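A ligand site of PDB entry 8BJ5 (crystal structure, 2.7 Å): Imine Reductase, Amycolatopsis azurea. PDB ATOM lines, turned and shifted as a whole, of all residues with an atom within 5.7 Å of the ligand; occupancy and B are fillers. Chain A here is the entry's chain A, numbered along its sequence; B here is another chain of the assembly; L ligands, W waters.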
ATOM      1  N   GLY A   8      -9.383   7.918 -15.338  1.00  0.00           N
ATOM      2  CA  GLY A   8      -8.763   9.207 -15.717  1.00  0.00           C
ATOM      3  C   GLY A   8      -7.521   9.466 -14.897  1.00  0.00           C
ATOM      4  O   GLY A   8      -7.677   9.816 -13.700  1.00  0.00           O
ATOM      5  N   LEU A   9      -6.345   9.307 -15.496  1.00  0.00           N
ATOM      6  CA  LEU A   9      -5.037   9.352 -14.786  1.00  0.00           C
ATOM      7  C   LEU A   9      -4.200  10.511 -15.322  1.00  0.00           C
ATOM      8  O   LEU A   9      -2.999  10.350 -15.551  1.00  0.00           O
ATOM      9  CB  LEU A   9      -4.350   7.996 -14.915  1.00  0.00           C
ATOM     10  CG  LEU A   9      -5.144   6.860 -14.279  1.00  0.00           C
ATOM     11  CD1 LEU A   9      -4.390   5.567 -14.328  1.00  0.00           C
ATOM     12  CD2 LEU A   9      -5.502   7.174 -12.829  1.00  0.00           C
ATOM     13  N   GLY A  10      -4.849  11.672 -15.464  1.00  0.00           N
ATOM     14  CA  GLY A  10      -4.160  12.976 -15.428  1.00  0.00           C
ATOM     15  C   GLY A  10      -3.539  13.201 -14.055  1.00  0.00           C
ATOM     16  O   GLY A  10      -3.653  12.364 -13.159  1.00  0.00           O
ATOM     17  N   PRO A  11      -2.861  14.342 -13.850  1.00  0.00           N
ATOM     18  CA  PRO A  11      -2.190  14.632 -12.580  1.00  0.00           C
ATOM     19  C   PRO A  11      -3.131  14.423 -11.389  1.00  0.00           C
ATOM     20  O   PRO A  11      -2.731  13.832 -10.399  1.00  0.00           O
ATOM     21  CB  PRO A  11      -1.794  16.120 -12.686  1.00  0.00           C
ATOM     22  CG  PRO A  11      -2.529  16.640 -13.932  1.00  0.00           C
ATOM     23  CD  PRO A  11      -2.730  15.438 -14.813  1.00  0.00           C
ATOM     24  N   MET A  12      -4.363  14.893 -11.538  1.00  0.00           N
ATOM     25  CA  MET A  12      -5.412  14.864 -10.492  1.00  0.00           C
ATOM     26  C   MET A  12      -5.721  13.395 -10.203  1.00  0.00           C
ATOM     27  O   MET A  12      -5.406  12.949  -9.089  1.00  0.00           O
ATOM     28  CB  MET A  12      -6.669  15.604 -10.957  1.00  0.00           C
ATOM     29  CG  MET A  12      -6.465  17.103 -11.196  1.00  0.00           C
ATOM     30  SD  MET A  12      -5.675  17.978  -9.819  1.00  0.00           S
ATOM     31  CE  MET A  12      -6.975  17.977  -8.593  1.00  0.00           C
ATOM     32  N   GLY A  13      -6.249  12.659 -11.183  1.00  0.00           N
ATOM     33  CA  GLY A  13      -6.565  11.217 -11.063  1.00  0.00           C
ATOM     34  C   GLY A  13      -5.447  10.521 -10.336  1.00  0.00           C
ATOM     35  O   GLY A  13      -5.716   9.888  -9.299  1.00  0.00           O
ATOM     36  N   TRP A  30      -8.361   2.431 -14.734  1.00  0.00           N
ATOM     37  CA  TRP A  30      -8.264   2.284 -16.213  1.00  0.00           C
ATOM     38  C   TRP A  30      -7.986   3.661 -16.782  1.00  0.00           C
ATOM     39  O   TRP A  30      -8.421   4.641 -16.152  1.00  0.00           O
ATOM     40  CB  TRP A  30      -9.552   1.694 -16.781  1.00  0.00           C
ATOM     41  CG  TRP A  30      -9.605   1.645 -18.276  1.00  0.00           C
ATOM     42  CD1 TRP A  30      -9.306   0.570 -19.064  1.00  0.00           C
ATOM     43  CD2 TRP A  30      -9.990   2.700 -19.166  1.00  0.00           C
ATOM     44  NE1 TRP A  30      -9.485   0.891 -20.379  1.00  0.00           N
ATOM     45  CE2 TRP A  30      -9.905   2.188 -20.485  1.00  0.00           C
ATOM     46  CE3 TRP A  30     -10.383   4.041 -19.004  1.00  0.00           C
ATOM     47  CZ2 TRP A  30     -10.213   2.944 -21.604  1.00  0.00           C
ATOM     48  CZ3 TRP A  30     -10.682   4.795 -20.127  1.00  0.00           C
ATOM     49  CH2 TRP A  30     -10.601   4.247 -21.410  1.00  0.00           C
ATOM     50  N   ASN A  31      -7.294   3.735 -17.925  1.00  0.00           N
ATOM     51  CA  ASN A  31      -7.098   5.012 -18.650  1.00  0.00           C
ATOM     52  C   ASN A  31      -6.937   4.728 -20.145  1.00  0.00           C
ATOM     53  O   ASN A  31      -6.344   3.711 -20.496  1.00  0.00           O
ATOM     54  CB  ASN A  31      -5.918   5.807 -18.102  1.00  0.00           C
ATOM     55  CG  ASN A  31      -5.974   7.260 -18.530  1.00  0.00           C
ATOM     56  OD1 ASN A  31      -7.043   7.872 -18.564  1.00  0.00           O
ATOM     57  ND2 ASN A  31      -4.820   7.815 -18.865  1.00  0.00           N
ATOM     58  N   ARG A  32      -7.475   5.619 -20.974  1.00  0.00           N
ATOM     59  CA  ARG A  32      -7.392   5.569 -22.459  1.00  0.00           C
ATOM     60  C   ARG A  32      -5.943   5.280 -22.879  1.00  0.00           C
ATOM     61  O   ARG A  32      -5.764   4.497 -23.846  1.00  0.00           O
ATOM     62  CB  ARG A  32      -7.922   6.892 -23.022  1.00  0.00           C
ATOM     63  CG  ARG A  32      -7.659   7.085 -24.509  1.00  0.00           C
ATOM     64  CD  ARG A  32      -8.188   8.411 -24.988  1.00  0.00           C
ATOM     65  NE  ARG A  32      -7.504   9.560 -24.383  1.00  0.00           N
ATOM     66  CZ  ARG A  32      -7.740  10.824 -24.698  1.00  0.00           C
ATOM     67  NH1 ARG A  32      -8.648  11.133 -25.607  1.00  0.00           N
ATOM     68  NH2 ARG A  32      -7.094  11.792 -24.069  1.00  0.00           N
ATOM     69  N   THR A  33      -4.962   5.860 -22.168  1.00  0.00           N
ATOM     70  CA  THR A  33      -3.500   5.692 -22.397  1.00  0.00           C
ATOM     71  C   THR A  33      -2.929   4.785 -21.309  1.00  0.00           C
ATOM     72  O   THR A  33      -2.470   5.339 -20.270  1.00  0.00           O
ATOM     73  CB  THR A  33      -2.819   7.063 -22.387  1.00  0.00           C
ATOM     74  OG1 THR A  33      -3.456   7.801 -23.417  1.00  0.00           O
ATOM     75  CG2 THR A  33      -1.339   7.060 -22.687  1.00  0.00           C
ATOM     76  N   ARG A  36       0.039   5.547 -18.850  1.00  0.00           N
ATOM     77  CA  ARG A  36       0.019   6.656 -17.844  1.00  0.00           C
ATOM     78  C   ARG A  36      -0.162   6.063 -16.441  1.00  0.00           C
ATOM     79  O   ARG A  36       0.222   6.758 -15.442  1.00  0.00           O
ATOM     80  CB  ARG A  36      -1.060   7.685 -18.175  1.00  0.00           C
ATOM     81  CG  ARG A  36      -0.554   8.930 -18.874  1.00  0.00           C
ATOM     82  CD  ARG A  36      -1.699   9.914 -18.936  1.00  0.00           C
ATOM     83  NE  ARG A  36      -1.327  11.252 -18.497  1.00  0.00           N
ATOM     84  CZ  ARG A  36      -2.084  12.336 -18.653  1.00  0.00           C
ATOM     85  NH1 ARG A  36      -3.282  12.254 -19.204  1.00  0.00           N
ATOM     86  NH2 ARG A  36      -1.651  13.517 -18.255  1.00  0.00           N
ATOM     87  N   SER A  64     -11.962  11.354 -13.185  1.00  0.00           N
ATOM     88  CA  SER A  64     -11.152  12.586 -13.330  1.00  0.00           C
ATOM     89  C   SER A  64     -10.819  12.801 -14.817  1.00  0.00           C
ATOM     90  O   SER A  64      -9.761  12.336 -15.248  1.00  0.00           O
ATOM     91  CB  SER A  64      -9.937  12.559 -12.457  1.00  0.00           C
ATOM     92  OG  SER A  64      -9.410  13.874 -12.336  1.00  0.00           O
ATOM     93  N   LEU A  65     -11.709  13.461 -15.557  1.00  0.00           N
ATOM     94  CA  LEU A  65     -11.638  13.559 -17.037  1.00  0.00           C
ATOM     95  C   LEU A  65     -11.770  15.014 -17.466  1.00  0.00           C
ATOM     96  O   LEU A  65     -12.394  15.794 -16.736  1.00  0.00           O
ATOM     97  CB  LEU A  65     -12.752  12.693 -17.632  1.00  0.00           C
ATOM     98  CG  LEU A  65     -12.736  11.227 -17.213  1.00  0.00           C
ATOM     99  CD1 LEU A  65     -13.978  10.516 -17.713  1.00  0.00           C
ATOM    100  CD2 LEU A  65     -11.474  10.532 -17.700  1.00  0.00           C
ATOM    101  N   THR A  66     -11.154  15.372 -18.588  1.00  0.00           N
ATOM    102  CA  THR A  66     -11.016  16.770 -19.079  1.00  0.00           C
ATOM    103  C   THR A  66     -12.401  17.424 -19.158  1.00  0.00           C
ATOM    104  O   THR A  66     -12.498  18.636 -18.817  1.00  0.00           O
ATOM    105  CB  THR A  66     -10.275  16.767 -20.417  1.00  0.00           C
ATOM    106  OG1 THR A  66      -9.106  15.975 -20.205  1.00  0.00           O
ATOM    107  CG2 THR A  66      -9.888  18.160 -20.887  1.00  0.00           C
ATOM    108  N   ASP A  67     -13.398  16.664 -19.595  1.00  0.00           N
ATOM    109  CA  ASP A  67     -14.802  17.107 -19.751  1.00  0.00           C
ATOM    110  C   ASP A  67     -15.742  15.917 -19.568  1.00  0.00           C
ATOM    111  O   ASP A  67     -15.254  14.779 -19.484  1.00  0.00           O
ATOM    112  CB  ASP A  67     -15.010  17.812 -21.088  1.00  0.00           C
ATOM    113  CG  ASP A  67     -14.659  17.015 -22.333  1.00  0.00           C
ATOM    114  OD1 ASP A  67     -14.690  15.760 -22.282  1.00  0.00           O
ATOM    115  OD2 ASP A  67     -14.366  17.679 -23.352  1.00  0.00           O
ATOM    116  N   ALA A  69     -18.098  14.936 -21.861  1.00  0.00           N
ATOM    117  CA  ALA A  69     -18.016  14.207 -23.158  1.00  0.00           C
ATOM    118  C   ALA A  69     -17.151  12.963 -23.007  1.00  0.00           C
ATOM    119  O   ALA A  69     -17.494  11.942 -23.618  1.00  0.00           O
ATOM    120  CB  ALA A  69     -17.493  15.099 -24.267  1.00  0.00           C
ATOM    121  N   ALA A  70     -16.062  13.046 -22.233  1.00  0.00           N
ATOM    122  CA  ALA A  70     -15.132  11.928 -21.955  1.00  0.00           C
ATOM    123  C   ALA A  70     -15.854  10.815 -21.177  1.00  0.00           C
ATOM    124  O   ALA A  70     -15.629   9.632 -21.486  1.00  0.00           O
ATOM    125  CB  ALA A  70     -13.930  12.422 -21.193  1.00  0.00           C
ATOM    126  N   ASP A  73     -17.787   8.713 -23.672  1.00  0.00           N
ATOM    127  CA  ASP A  73     -16.873   7.895 -24.506  1.00  0.00           C
ATOM    128  C   ASP A  73     -16.481   6.633 -23.741  1.00  0.00           C
ATOM    129  O   ASP A  73     -16.471   5.550 -24.369  1.00  0.00           O
ATOM    130  CB  ASP A  73     -15.620   8.683 -24.905  1.00  0.00           C
ATOM    131  CG  ASP A  73     -15.841   9.821 -25.892  1.00  0.00           C
ATOM    132  OD1 ASP A  73     -16.949   9.909 -26.471  1.00  0.00           O
ATOM    133  OD2 ASP A  73     -14.910  10.637 -26.069  1.00  0.00           O
ATOM    134  N   ILE A  74     -16.206   6.755 -22.442  1.00  0.00           N
ATOM    135  CA  ILE A  74     -15.659   5.665 -21.570  1.00  0.00           C
ATOM    136  C   ILE A  74     -16.804   4.812 -21.030  1.00  0.00           C
ATOM    137  O   ILE A  74     -16.781   3.584 -21.299  1.00  0.00           O
ATOM    138  CB  ILE A  74     -14.821   6.262 -20.425  1.00  0.00           C
ATOM    139  CG1 ILE A  74     -13.639   7.057 -20.979  1.00  0.00           C
ATOM    140  CG2 ILE A  74     -14.377   5.184 -19.431  1.00  0.00           C
ATOM    141  CD1 ILE A  74     -13.048   8.047 -20.000  1.00  0.00           C
ATOM    142  N   LEU A  90     -15.552  14.070 -11.026  1.00  0.00           N
ATOM    143  CA  LEU A  90     -14.736  15.223 -10.560  1.00  0.00           C
ATOM    144  C   LEU A  90     -14.175  15.993 -11.759  1.00  0.00           C
ATOM    145  O   LEU A  90     -13.122  16.649 -11.627  1.00  0.00           O
ATOM    146  CB  LEU A  90     -13.649  14.679  -9.630  1.00  0.00           C
ATOM    147  CG  LEU A  90     -14.180  13.874  -8.448  1.00  0.00           C
ATOM    148  CD1 LEU A  90     -13.040  13.414  -7.566  1.00  0.00           C
ATOM    149  CD2 LEU A  90     -15.151  14.675  -7.609  1.00  0.00           C
ATOM    150  N   SER A  91     -14.894  15.927 -12.880  1.00  0.00           N
ATOM    151  CA  SER A  91     -14.556  16.590 -14.174  1.00  0.00           C
ATOM    152  C   SER A  91     -15.240  17.958 -14.234  1.00  0.00           C
ATOM    153  O   SER A  91     -16.368  18.074 -13.741  1.00  0.00           O
ATOM    154  CB  SER A  91     -14.958  15.731 -15.351  1.00  0.00           C
ATOM    155  OG  SER A  91     -14.510  14.390 -15.207  1.00  0.00           O
ATOM    156  N   SER A  92     -14.560  18.944 -14.830  1.00  0.00           N
ATOM    157  CA  SER A  92     -15.156  20.233 -15.266  1.00  0.00           C
ATOM    158  C   SER A  92     -16.029  19.994 -16.493  1.00  0.00           C
ATOM    159  O   SER A  92     -15.606  19.257 -17.394  1.00  0.00           O
ATOM    160  CB  SER A  92     -14.117  21.282 -15.540  1.00  0.00           C
ATOM    161  OG  SER A  92     -14.708  22.477 -16.026  1.00  0.00           O
ATOM    162  N   VAL A 117     -12.867  19.660  -7.480  1.00  0.00           N
ATOM    163  CA  VAL A 117     -11.672  19.659  -6.589  1.00  0.00           C
ATOM    164  C   VAL A 117     -10.964  21.000  -6.744  1.00  0.00           C
ATOM    165  O   VAL A 117     -10.637  21.364  -7.879  1.00  0.00           O
ATOM    166  CB  VAL A 117     -10.745  18.467  -6.917  1.00  0.00           C
ATOM    167  CG1 VAL A 117      -9.628  18.334  -5.906  1.00  0.00           C
ATOM    168  CG2 VAL A 117     -11.515  17.155  -7.046  1.00  0.00           C
ATOM    169  N   MET A 118     -10.739  21.726  -5.638  1.00  0.00           N
ATOM    170  CA  MET A 118     -10.403  23.167  -5.652  1.00  0.00           C
ATOM    171  C   MET A 118      -8.954  23.401  -5.238  1.00  0.00           C
ATOM    172  O   MET A 118      -8.651  24.458  -4.608  1.00  0.00           O
ATOM    173  CB  MET A 118     -11.350  23.931  -4.735  1.00  0.00           C
ATOM    174  CG  MET A 118     -12.614  24.275  -5.455  1.00  0.00           C
ATOM    175  SD  MET A 118     -12.216  25.264  -6.932  1.00  0.00           S
ATOM    176  CE  MET A 118     -13.723  24.950  -7.811  1.00  0.00           C
ATOM    177  N   VAL A 119      -8.080  22.484  -5.651  1.00  0.00           N
ATOM    178  CA  VAL A 119      -6.619  22.538  -5.361  1.00  0.00           C
ATOM    179  C   VAL A 119      -5.880  21.907  -6.542  1.00  0.00           C
ATOM    180  O   VAL A 119      -6.467  21.097  -7.273  1.00  0.00           O
ATOM    181  CB  VAL A 119      -6.313  21.833  -4.023  1.00  0.00           C
ATOM    182  CG1 VAL A 119      -6.621  22.732  -2.835  1.00  0.00           C
ATOM    183  CG2 VAL A 119      -6.988  20.471  -3.912  1.00  0.00           C
ATOM    184  N   PRO A 120      -4.614  22.305  -6.815  1.00  0.00           N
ATOM    185  CA  PRO A 120      -3.784  21.582  -7.775  1.00  0.00           C
ATOM    186  C   PRO A 120      -3.366  20.205  -7.215  1.00  0.00           C
ATOM    187  O   PRO A 120      -3.392  20.026  -5.996  1.00  0.00           O
ATOM    188  CB  PRO A 120      -2.570  22.511  -7.984  1.00  0.00           C
ATOM    189  CG  PRO A 120      -2.524  23.380  -6.741  1.00  0.00           C
ATOM    190  CD  PRO A 120      -3.932  23.469  -6.223  1.00  0.00           C
ATOM    191  N   ALA A 121      -2.989  19.267  -8.099  1.00  0.00           N
ATOM    192  CA  ALA A 121      -2.688  17.858  -7.764  1.00  0.00           C
ATOM    193  C   ALA A 121      -1.667  17.800  -6.618  1.00  0.00           C
ATOM    194  O   ALA A 121      -1.809  16.926  -5.746  1.00  0.00           O
ATOM    195  CB  ALA A 121      -2.184  17.114  -8.984  1.00  0.00           C
ATOM    196  N   TYR A 167     -17.676  25.116  -9.009  1.00  0.00           N
ATOM    197  CA  TYR A 167     -16.365  24.857  -9.655  1.00  0.00           C
ATOM    198  C   TYR A 167     -16.150  25.904 -10.768  1.00  0.00           C
ATOM    199  O   TYR A 167     -15.136  26.643 -10.720  1.00  0.00           O
ATOM    200  CB  TYR A 167     -16.218  23.406 -10.133  1.00  0.00           C
ATOM    201  CG  TYR A 167     -14.831  23.097 -10.645  1.00  0.00           C
ATOM    202  CD1 TYR A 167     -13.846  22.658  -9.779  1.00  0.00           C
ATOM    203  CD2 TYR A 167     -14.478  23.316 -11.973  1.00  0.00           C
ATOM    204  CE1 TYR A 167     -12.547  22.423 -10.220  1.00  0.00           C
ATOM    205  CE2 TYR A 167     -13.189  23.099 -12.423  1.00  0.00           C
ATOM    206  CZ  TYR A 167     -12.212  22.646 -11.540  1.00  0.00           C
ATOM    207  OH  TYR A 167     -10.939  22.410 -11.964  1.00  0.00           O
ATOM    208  N   LEU A 171     -13.114  28.759 -11.032  1.00  0.00           N
ATOM    209  CA  LEU A 171     -12.192  28.769 -12.193  1.00  0.00           C
ATOM    210  C   LEU A 171     -12.432  30.036 -13.021  1.00  0.00           C
ATOM    211  O   LEU A 171     -11.448  30.534 -13.588  1.00  0.00           O
ATOM    212  CB  LEU A 171     -12.354  27.468 -12.979  1.00  0.00           C
ATOM    213  CG  LEU A 171     -11.378  26.376 -12.487  1.00  0.00           C
ATOM    214  CD1 LEU A 171     -11.762  25.822 -11.118  1.00  0.00           C
ATOM    215  CD2 LEU A 171     -11.242  25.272 -13.505  1.00  0.00           C
ATOM    216  N   GLU B 229       1.594  18.809 -14.662  1.00  0.00           N
ATOM    217  CA  GLU B 229       0.639  19.047 -13.545  1.00  0.00           C
ATOM    218  C   GLU B 229      -0.713  19.620 -14.024  1.00  0.00           C
ATOM    219  O   GLU B 229      -1.690  19.463 -13.285  1.00  0.00           O
ATOM    220  CB  GLU B 229       1.240  20.035 -12.540  1.00  0.00           C
ATOM    221  CG  GLU B 229       2.510  19.540 -11.893  1.00  0.00           C
ATOM    222  CD  GLU B 229       2.339  18.296 -11.038  1.00  0.00           C
ATOM    223  OE1 GLU B 229       1.612  18.372 -10.008  1.00  0.00           O
ATOM    224  OE2 GLU B 229       2.937  17.236 -11.411  1.00  0.00           O
ATOM    225  N   ALA B 230      -0.768  20.271 -15.197  1.00  0.00           N
ATOM    226  CA  ALA B 230      -1.968  20.971 -15.718  1.00  0.00           C
ATOM    227  C   ALA B 230      -1.641  21.596 -17.073  1.00  0.00           C
ATOM    228  O   ALA B 230      -0.786  22.511 -17.135  1.00  0.00           O
ATOM    229  CB  ALA B 230      -2.431  22.056 -14.770  1.00  0.00           C
ATOM    230  N   ASP B 231      -2.329  21.129 -18.130  1.00  0.00           N
ATOM    231  CA  ASP B 231      -1.994  21.499 -19.525  1.00  0.00           C
ATOM    232  C   ASP B 231      -3.075  22.428 -20.087  1.00  0.00           C
ATOM    233  O   ASP B 231      -4.191  22.524 -19.525  1.00  0.00           O
ATOM    234  CB  ASP B 231      -1.717  20.249 -20.361  1.00  0.00           C
ATOM    235  CG  ASP B 231      -2.916  19.402 -20.764  1.00  0.00           C
ATOM    236  OD1 ASP B 231      -4.049  19.717 -20.360  1.00  0.00           O
ATOM    237  OD2 ASP B 231      -2.697  18.415 -21.496  1.00  0.00           O
ATOM    238  N   MET B 234      -6.655  20.931 -20.968  1.00  0.00           N
ATOM    239  CA  MET B 234      -7.594  20.774 -19.826  1.00  0.00           C
ATOM    240  C   MET B 234      -8.104  22.161 -19.402  1.00  0.00           C
ATOM    241  O   MET B 234      -9.311  22.258 -19.155  1.00  0.00           O
ATOM    242  CB  MET B 234      -6.945  20.036 -18.656  1.00  0.00           C
ATOM    243  CG  MET B 234      -7.621  20.227 -17.306  1.00  0.00           C
ATOM    244  SD  MET B 234      -6.738  21.571 -16.495  1.00  0.00           S
ATOM    245  CE  MET B 234      -7.967  22.305 -15.416  1.00  0.00           C
ATOM    246  N   SER B 238     -11.800  23.980 -19.484  1.00  0.00           N
ATOM    247  CA  SER B 238     -12.345  24.728 -18.316  1.00  0.00           C
ATOM    248  C   SER B 238     -12.881  26.071 -18.821  1.00  0.00           C
ATOM    249  O   SER B 238     -14.053  26.398 -18.523  1.00  0.00           O
ATOM    250  CB  SER B 238     -11.311  24.916 -17.237  1.00  0.00           C
ATOM    251  OG  SER B 238     -11.356  23.845 -16.319  1.00  0.00           O
ATOM    252  N   ARG B 273      -0.293  20.932 -24.901  1.00  0.00           N
ATOM    253  CA  ARG B 273       0.279  19.999 -23.908  1.00  0.00           C
ATOM    254  C   ARG B 273       1.217  20.769 -22.962  1.00  0.00           C
ATOM    255  O   ARG B 273       1.649  20.178 -21.946  1.00  0.00           O
ATOM    256  CB  ARG B 273       0.938  18.843 -24.656  1.00  0.00           C
ATOM    257  CG  ARG B 273       1.287  17.624 -23.802  1.00  0.00           C
ATOM    258  CD  ARG B 273       0.145  16.888 -23.120  1.00  0.00           C
ATOM    259  NE  ARG B 273      -0.822  16.356 -24.073  1.00  0.00           N
ATOM    260  CZ  ARG B 273      -1.892  15.646 -23.749  1.00  0.00           C
ATOM    261  NH1 ARG B 273      -2.124  15.337 -22.484  1.00  0.00           N
ATOM    262  NH2 ARG B 273      -2.714  15.219 -24.691  1.00  0.00           N
HETATM  263  P1  LIG L   1      -6.696  16.218 -18.084  1.00  0.00           P
HETATM  264  O1  LIG L   1      -5.531  16.755 -18.850  1.00  0.00           O
HETATM  265  O2  LIG L   1      -7.922  17.055 -17.965  1.00  0.00           O
HETATM  266  O3  LIG L   1      -7.102  14.745 -18.617  1.00  0.00           O
HETATM  267  C1  LIG L   1      -7.341  13.757 -17.571  1.00  0.00           C
HETATM  268  C2  LIG L   1      -7.832  12.450 -18.159  1.00  0.00           C
HETATM  269  O4  LIG L   1      -8.868  12.673 -19.152  1.00  0.00           O
HETATM  270  C3  LIG L   1      -6.764  11.594 -18.858  1.00  0.00           C
HETATM  271  O5  LIG L   1      -6.663  10.354 -18.150  1.00  0.00           O
HETATM  272  C4  LIG L   1      -7.249  11.552 -20.314  1.00  0.00           C
HETATM  273  O6  LIG L   1      -6.928  10.368 -21.046  1.00  0.00           O
HETATM  274  C5  LIG L   1      -8.752  11.643 -20.094  1.00  0.00           C
HETATM  275  N1  LIG L   1      -9.575  11.941 -21.279  1.00  0.00           N
HETATM  276  C6  LIG L   1      -9.829  13.173 -21.818  1.00  0.00           C
HETATM  277  N2  LIG L   1     -10.636  13.144 -22.849  1.00  0.00           N
HETATM  278  C7  LIG L   1     -10.945  11.798 -23.010  1.00  0.00           C
HETATM  279  C8  LIG L   1     -11.760  11.109 -23.938  1.00  0.00           C
HETATM  280  N3  LIG L   1     -12.467  11.714 -24.881  1.00  0.00           N
HETATM  281  N4  LIG L   1     -11.839   9.768 -23.826  1.00  0.00           N
HETATM  282  C9  LIG L   1     -11.150   9.165 -22.846  1.00  0.00           C
HETATM  283  N5  LIG L   1     -10.367   9.695 -21.916  1.00  0.00           N
HETATM  284  C10 LIG L   1     -10.293  11.044 -22.048  1.00  0.00           C
HETATM  285  O7  LIG L   1      -6.180  15.847 -16.611  1.00  0.00           O
HETATM  286  P2  LIG L   1      -6.216  16.621 -15.220  1.00  0.00           P
HETATM  287  O8  LIG L   1      -5.551  17.950 -15.368  1.00  0.00           O
HETATM  288  O9  LIG L   1      -5.718  15.723 -14.126  1.00  0.00           O
HETATM  289  O10 LIG L   1      -7.791  16.774 -15.103  1.00  0.00           O
HETATM  290  C11 LIG L   1      -8.337  16.843 -13.777  1.00  0.00           C
HETATM  291  C12 LIG L   1      -9.809  17.132 -13.857  1.00  0.00           C
HETATM  292  O11 LIG L   1     -10.187  17.880 -12.683  1.00  0.00           O
HETATM  293  C13 LIG L   1     -10.249  18.020 -15.019  1.00  0.00           C
HETATM  294  O12 LIG L   1     -11.637  17.869 -15.294  1.00  0.00           O
HETATM  295  C14 LIG L   1      -9.893  19.409 -14.484  1.00  0.00           C
HETATM  296  O13 LIG L   1     -10.733  20.387 -15.070  1.00  0.00           O
HETATM  297  C15 LIG L   1     -10.135  19.276 -12.976  1.00  0.00           C
HETATM  298  N6  LIG L   1      -9.093  19.895 -12.102  1.00  0.00           N
HETATM  299  C16 LIG L   1      -7.780  20.084 -12.507  1.00  0.00           C
HETATM  300  C17 LIG L   1      -6.839  20.639 -11.633  1.00  0.00           C
HETATM  301  C18 LIG L   1      -5.402  20.808 -12.049  1.00  0.00           C
HETATM  302  O14 LIG L   1      -4.583  21.239 -11.226  1.00  0.00           O
HETATM  303  N7  LIG L   1      -5.088  20.476 -13.296  1.00  0.00           N
HETATM  304  C19 LIG L   1      -7.228  21.045 -10.365  1.00  0.00           C
HETATM  305  C20 LIG L   1      -8.533  20.943 -10.013  1.00  0.00           C
HETATM  306  C21 LIG L   1      -9.415  20.258 -10.833  1.00  0.00           C
HETATM  307  P3  LIG L   1      -5.366  10.292 -21.430  1.00  0.00           P
HETATM  308  O15 LIG L   1      -4.545  10.317 -20.169  1.00  0.00           O
HETATM  309  O16 LIG L   1      -5.297   8.952 -22.109  1.00  0.00           O
HETATM  310  O17 LIG L   1      -5.042  11.438 -22.345  1.00  0.00           O
HETATM  311  O   HOH W   1     -10.554   8.715 -26.396  1.00  0.00           O
HETATM  312  O   HOH W   2      -5.155  14.269 -22.004  1.00  0.00           O
HETATM  313  O   HOH W   3      -4.318  19.313 -17.697  1.00  0.00           O
HETATM  314  O   HOH W   4     -12.296  18.666  -9.952  1.00  0.00           O
HETATM  315  O   HOH W   5     -12.778  14.909 -24.371  1.00  0.00           O
HETATM  316  O   HOH W   6      -6.878  13.412 -13.860  1.00  0.00           O
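N of Leu 9 lies within hydrogen-bond range of O5 of the ligand, at 2.9 Å. An oxygen (O17) of the ligand lies within salt-bridge range of the guanidinium group of Arg 32 (2.7 Å). O2 of the ligand sits at hydrogen-bond distance from OG1 of Thr 66 (2.8 Å). The side-chain amide oxygen (OD1) of Asn 31 sits at hydrogen-bond distance from an oxygen (O5) of the ligand, at 2.5 Å. The side-chain sulfur (SD) of Met 234 of chain B lies within hydrogen-bond range of a nitrogen (N7) of the ligand (3.8 Å). N of Thr 33 lies within hydrogen-bond range of O16 of the ligand (3.1 Å). O12 of the ligand sits at hydrogen-bond distance from O of Leu 65 (2.6 Å). The side-chain carboxylate (OD2) of Asp 73 sits at hydrogen-bond distance from a nitrogen (N3) of the ligand (2.9 Å). An oxygen (O16) of the ligand lies within hydrogen-bond range of the side-chain hydroxyl (OG1) of Thr 33 (2.5 Å). The backbone NH (N) of Ser 92 sits at hydrogen-bond distance from an oxygen (O12) of the ligand (3.1 Å). O15 of the ligand lies within salt-bridge range of NH1 of Arg 36 (2.5 Å). The backbone NH (N) of Met 12 sits at hydrogen-bond distance from an oxygen (O9) of the ligand (3.0 Å). An oxygen (O5) of the ligand is in hydrogen-bond range of the backbone NH (N) of Gly 10 (3.5 Å).
The backbone NH (N) of Ala 70 lies within hydrogen-bond range of the side-chain carboxylate (OD1) of Asp 67, 3.0 Å away. OD2 of Asp 231 of chain B is in salt-bridge range of NH1 of Arg 273 of chain B, at 3.3 Å. The side-chain sulfur (SD) of Met 12 lies within hydrogen-bond range of the backbone NH (N) of Ala 121, 3.4 Å away. The backbone NH (N) of Met 234 of chain B sits at hydrogen-bond distance from the side-chain carboxylate (OD1) of Asp 231 of chain B. OG of Ser 91 sits close to O of Leu 65 (3.0 Å). The side-chain amide oxygen (OD1) of Asn 31 sits at hydrogen-bond distance from the backbone NH (N) of Leu 9, at 3.5 Å.
An oxygen (O9) of the ligand sits close to the backbone nitrogen (N) of Pro 11 (3.2 Å). O of Leu 90 sits close to O11 of the ligand (3.4 Å). OH of Tyr 167 lies close to N6 of the ligand, 3.1 Å away. CA of Gly 8 touches O5 of the ligand, 3.4 Å away. Ser 64 touches the ligand. Ala 70 touches the ligand. Ile 74 touches the ligand. Ser 91 touches the ligand (CA to O12, 3.4 Å). Val 117 touches the ligand (O to C20, 3.0 Å). O of Val 119 touches C19 of the ligand, 3.2 Å away. Pro 120 touches the ligand (CA to O14, 3.6 Å). Glu 229 of chain B touches the ligand (O to N7, 3.5 Å). CB of Ala 230 of chain B touches N7 of the ligand, at 3.4 Å. Asp 231 of chain B touches the ligand. Ser 238 of chain B touches the ligand. Hydrophobic or aromatic side chains that line the ligand: Pro 11, Met 12, Leu 65, Ala 70, Ile 74, Tyr 167, Ala 230 of chain B and Met 234 of chain B.
Water W6 lies within hydrogen-bond range of an oxygen (O9) of the ligand, the backbone NH of Gly 13, the side-chain hydroxyl of Ser 64 and the backbone NH of Gly 10. Water W2 bridges an oxygen (O17) of the ligand (2.9 Å) and the guanidinium group (NH1) of Arg 273 of chain B (3.2 Å). Water W3 lies within hydrogen-bond range of the side-chain carboxylate of Asp 231 of chain B, an oxygen (O8) of the ligand and the side-chain sulfur of Met 234 of chain B. Water W1 bridges a nitrogen (N4) of the ligand (3.1 Å) and the guanidinium group (NH1) of Arg 32 (3.2 Å). Water W5 bridges OD1 of Asp 67 (3.0 Å) and N2 of the ligand (3.2 Å). Water W4 bridges N of Val 117 (2.7 Å) and O of Leu 90 (2.7 Å).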
